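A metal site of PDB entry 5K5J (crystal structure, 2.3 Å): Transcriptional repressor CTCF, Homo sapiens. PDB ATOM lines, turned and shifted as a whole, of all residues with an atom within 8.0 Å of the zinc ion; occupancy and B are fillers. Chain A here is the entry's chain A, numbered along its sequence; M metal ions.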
ATOM      1  N   LYS A  96     -13.420  29.105   4.239  1.00  0.00           N
ATOM      2  CA  LYS A  96     -13.153  28.760   5.629  1.00  0.00           C
ATOM      3  C   LYS A  96     -13.609  27.346   5.916  1.00  0.00           C
ATOM      4  O   LYS A  96     -14.686  26.921   5.485  1.00  0.00           O
ATOM      5  CB  LYS A  96     -13.850  29.732   6.582  1.00  0.00           C
ATOM      6  CG  LYS A  96     -13.485  29.533   8.047  1.00  0.00           C
ATOM      7  CD  LYS A  96     -14.370  30.341   8.967  1.00  0.00           C
ATOM      8  CE  LYS A  96     -15.672  29.617   9.295  1.00  0.00           C
ATOM      9  NZ  LYS A  96     -15.469  28.539  10.299  1.00  0.00           N
ATOM     10  N   CYS A  97     -12.777  26.603   6.644  1.00  0.00           N
ATOM     11  CA  CYS A  97     -13.188  25.306   7.177  1.00  0.00           C
ATOM     12  C   CYS A  97     -14.465  25.462   7.992  1.00  0.00           C
ATOM     13  O   CYS A  97     -14.627  26.427   8.747  1.00  0.00           O
ATOM     14  CB  CYS A  97     -12.074  24.717   8.048  1.00  0.00           C
ATOM     15  SG  CYS A  97     -12.476  23.156   8.864  1.00  0.00           S
ATOM     16  N   ARG A  98     -15.383  24.518   7.836  1.00  0.00           N
ATOM     17  CA  ARG A  98     -16.637  24.564   8.568  1.00  0.00           C
ATOM     18  C   ARG A  98     -16.504  24.098  10.014  1.00  0.00           C
ATOM     19  O   ARG A  98     -17.504  24.109  10.741  1.00  0.00           O
ATOM     20  CB  ARG A  98     -17.705  23.737   7.845  1.00  0.00           C
ATOM     21  CG  ARG A  98     -17.341  22.284   7.617  1.00  0.00           C
ATOM     22  CD  ARG A  98     -18.455  21.521   6.915  1.00  0.00           C
ATOM     23  NE  ARG A  98     -19.678  21.477   7.711  1.00  0.00           N
ATOM     24  CZ  ARG A  98     -20.794  20.874   7.324  1.00  0.00           C
ATOM     25  NH1 ARG A  98     -20.863  20.262   6.144  1.00  0.00           N
ATOM     26  NH2 ARG A  98     -21.866  20.882   8.122  1.00  0.00           N
ATOM     27  N   TYR A  99     -15.311  23.698  10.437  1.00  0.00           N
ATOM     28  CA  TYR A  99     -15.081  23.262  11.803  1.00  0.00           C
ATOM     29  C   TYR A  99     -14.064  24.101  12.563  1.00  0.00           C
ATOM     30  O   TYR A  99     -14.004  23.999  13.798  1.00  0.00           O
ATOM     31  CB  TYR A  99     -14.620  21.790  11.822  1.00  0.00           C
ATOM     32  CG  TYR A  99     -15.540  20.857  11.051  1.00  0.00           C
ATOM     33  CD1 TYR A  99     -16.779  20.493  11.565  1.00  0.00           C
ATOM     34  CD2 TYR A  99     -15.157  20.343   9.818  1.00  0.00           C
ATOM     35  CE1 TYR A  99     -17.615  19.635  10.855  1.00  0.00           C
ATOM     36  CE2 TYR A  99     -15.993  19.486   9.108  1.00  0.00           C
ATOM     37  CZ  TYR A  99     -17.220  19.146   9.632  1.00  0.00           C
ATOM     38  OH  TYR A  99     -18.053  18.294   8.935  1.00  0.00           O
ATOM     39  N   CYS A 100     -13.269  24.921  11.882  1.00  0.00           N
ATOM     40  CA  CYS A 100     -12.324  25.812  12.548  1.00  0.00           C
ATOM     41  C   CYS A 100     -12.157  27.059  11.687  1.00  0.00           C
ATOM     42  O   CYS A 100     -12.859  27.245  10.686  1.00  0.00           O
ATOM     43  CB  CYS A 100     -10.982  25.108  12.789  1.00  0.00           C
ATOM     44  SG  CYS A 100      -9.939  24.908  11.321  1.00  0.00           S
ATOM     45  N   ASP A 101     -11.227  27.929  12.068  1.00  0.00           N
ATOM     46  CA  ASP A 101     -11.065  29.219  11.400  1.00  0.00           C
ATOM     47  C   ASP A 101     -10.016  29.197  10.284  1.00  0.00           C
ATOM     48  O   ASP A 101      -9.636  30.266   9.792  1.00  0.00           O
ATOM     49  CB  ASP A 101     -10.715  30.309  12.429  1.00  0.00           C
ATOM     50  CG  ASP A 101      -9.484  29.979  13.252  1.00  0.00           C
ATOM     51  OD1 ASP A 101      -8.662  29.140  12.811  1.00  0.00           O
ATOM     52  OD2 ASP A 101      -9.325  30.566  14.346  1.00  0.00           O
ATOM     53  N   ALA A 102      -9.533  28.022   9.898  1.00  0.00           N
ATOM     54  CA  ALA A 102      -8.540  27.938   8.828  1.00  0.00           C
ATOM     55  C   ALA A 102      -9.180  28.266   7.489  1.00  0.00           C
ATOM     56  O   ALA A 102     -10.289  27.808   7.179  1.00  0.00           O
ATOM     57  CB  ALA A 102      -7.901  26.563   8.793  1.00  0.00           C
ATOM     58  N   VAL A 103      -8.467  29.052   6.675  1.00  0.00           N
ATOM     59  CA  VAL A 103      -8.944  29.474   5.364  1.00  0.00           C
ATOM     60  C   VAL A 103      -8.007  28.926   4.299  1.00  0.00           C
ATOM     61  O   VAL A 103      -6.784  28.932   4.481  1.00  0.00           O
ATOM     62  CB  VAL A 103      -9.053  31.008   5.272  1.00  0.00           C
ATOM     63  CG1 VAL A 103      -9.358  31.450   3.840  1.00  0.00           C
ATOM     64  CG2 VAL A 103     -10.134  31.494   6.204  1.00  0.00           C
ATOM     65  N   PHE A 104      -8.588  28.463   3.207  1.00  0.00           N
ATOM     66  CA  PHE A 104      -7.828  27.920   2.089  1.00  0.00           C
ATOM     67  C   PHE A 104      -8.277  28.586   0.794  1.00  0.00           C
ATOM     68  O   PHE A 104      -9.368  29.172   0.724  1.00  0.00           O
ATOM     69  CB  PHE A 104      -7.992  26.397   2.005  1.00  0.00           C
ATOM     70  CG  PHE A 104      -7.536  25.675   3.252  1.00  0.00           C
ATOM     71  CD1 PHE A 104      -6.250  25.181   3.345  1.00  0.00           C
ATOM     72  CD2 PHE A 104      -8.396  25.541   4.334  1.00  0.00           C
ATOM     73  CE1 PHE A 104      -5.828  24.541   4.494  1.00  0.00           C
ATOM     74  CE2 PHE A 104      -7.975  24.901   5.483  1.00  0.00           C
ATOM     75  CZ  PHE A 104      -6.690  24.401   5.563  1.00  0.00           C
ATOM     76  N   LEU A 110      -9.215  22.798   0.953  1.00  0.00           N
ATOM     77  CA  LEU A 110     -10.315  22.909   1.916  1.00  0.00           C
ATOM     78  C   LEU A 110     -10.877  21.532   2.279  1.00  0.00           C
ATOM     79  O   LEU A 110     -11.054  21.218   3.456  1.00  0.00           O
ATOM     80  CB  LEU A 110     -11.414  23.794   1.330  1.00  0.00           C
ATOM     81  CG  LEU A 110     -12.691  23.928   2.170  1.00  0.00           C
ATOM     82  CD1 LEU A 110     -12.459  24.847   3.358  1.00  0.00           C
ATOM     83  CD2 LEU A 110     -13.853  24.406   1.309  1.00  0.00           C
ATOM     84  N   HIS A 113      -8.367  19.326   4.301  1.00  0.00           N
ATOM     85  CA  HIS A 113      -8.240  19.779   5.677  1.00  0.00           C
ATOM     86  C   HIS A 113      -9.455  19.393   6.507  1.00  0.00           C
ATOM     87  O   HIS A 113      -9.329  18.897   7.623  1.00  0.00           O
ATOM     88  CB  HIS A 113      -8.027  21.288   5.734  1.00  0.00           C
ATOM     89  CG  HIS A 113      -8.228  21.870   7.098  1.00  0.00           C
ATOM     90  ND1 HIS A 113      -7.243  21.874   8.063  1.00  0.00           N
ATOM     91  CD2 HIS A 113      -9.313  22.457   7.667  1.00  0.00           C
ATOM     92  CE1 HIS A 113      -7.703  22.447   9.161  1.00  0.00           C
ATOM     93  NE2 HIS A 113      -8.959  22.803   8.957  1.00  0.00           N
ATOM     94  N   GLN A 114     -10.656  19.643   5.962  1.00  0.00           N
ATOM     95  CA  GLN A 114     -11.880  19.318   6.682  1.00  0.00           C
ATOM     96  C   GLN A 114     -11.927  17.848   7.082  1.00  0.00           C
ATOM     97  O   GLN A 114     -12.470  17.499   8.137  1.00  0.00           O
ATOM     98  CB  GLN A 114     -13.107  19.676   5.846  1.00  0.00           C
ATOM     99  CG  GLN A 114     -13.438  21.158   5.813  1.00  0.00           C
ATOM    100  CD  GLN A 114     -14.713  21.450   5.053  1.00  0.00           C
ATOM    101  OE1 GLN A 114     -15.280  22.540   5.164  1.00  0.00           O
ATOM    102  NE2 GLN A 114     -15.180  20.472   4.281  1.00  0.00           N
ATOM    103  N   LYS A 115     -11.369  16.961   6.246  1.00  0.00           N
ATOM    104  CA  LYS A 115     -11.329  15.544   6.584  1.00  0.00           C
ATOM    105  C   LYS A 115     -10.450  15.253   7.789  1.00  0.00           C
ATOM    106  O   LYS A 115     -10.662  14.230   8.455  1.00  0.00           O
ATOM    107  CB  LYS A 115     -10.834  14.733   5.376  1.00  0.00           C
ATOM    108  CG  LYS A 115     -11.874  14.557   4.284  1.00  0.00           C
ATOM    109  CD  LYS A 115     -11.344  13.667   3.165  1.00  0.00           C
ATOM    110  CE  LYS A 115     -12.414  13.417   2.119  1.00  0.00           C
ATOM    111  NZ  LYS A 115     -11.870  12.657   0.958  1.00  0.00           N
ATOM    112  N   SER A 116      -9.490  16.113   8.098  1.00  0.00           N
ATOM    113  CA  SER A 116      -8.626  15.876   9.252  1.00  0.00           C
ATOM    114  C   SER A 116      -9.358  16.036  10.566  1.00  0.00           C
ATOM    115  O   SER A 116      -8.890  15.540  11.598  1.00  0.00           O
ATOM    116  CB  SER A 116      -7.405  16.803   9.206  1.00  0.00           C
ATOM    117  OG  SER A 116      -7.780  18.134   9.512  1.00  0.00           O
ATOM    118  N   HIS A 117     -10.498  16.725  10.571  1.00  0.00           N
ATOM    119  CA  HIS A 117     -11.316  16.845  11.771  1.00  0.00           C
ATOM    120  C   HIS A 117     -12.087  15.539  12.021  1.00  0.00           C
ATOM    121  O   HIS A 117     -11.962  14.934  13.081  1.00  0.00           O
ATOM    122  CB  HIS A 117     -12.301  18.011  11.644  1.00  0.00           C
ATOM    123  CG  HIS A 117     -11.640  19.357  11.673  1.00  0.00           C
ATOM    124  ND1 HIS A 117     -11.187  19.944  12.833  1.00  0.00           N
ATOM    125  CD2 HIS A 117     -11.354  20.225  10.676  1.00  0.00           C
ATOM    126  CE1 HIS A 117     -10.662  21.127  12.552  1.00  0.00           C
ATOM    127  NE2 HIS A 117     -10.742  21.317  11.245  1.00  0.00           N
HETATM  128 ZN    ZN M   1     -10.566  23.062  10.209  1.00  0.00          ZN
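O of His 113 lies within hydrogen-bond range of OG of Ser 116. N of Ala 102 lies close to SG of Cys 100. The side-chain amino group (NZ) of Lys 96 lies within hydrogen-bond range of the backbone carbonyl oxygen (O) of Cys 100. The side-chain sulfur (SG) of Cys 97 sits close to the backbone NH (N) of Tyr 99 (3.3 Å). The backbone NH of Cys 97 lies within hydrogen-bond range of the backbone carbonyl oxygen of Ala 102, at 2.8 Å.
The zinc ion is bound by a ring nitrogen (NE2) of His 117, a ring nitrogen (NE2) of His 113, the side-chain sulfur of Cys 100 and the side-chain sulfur of Cys 97.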
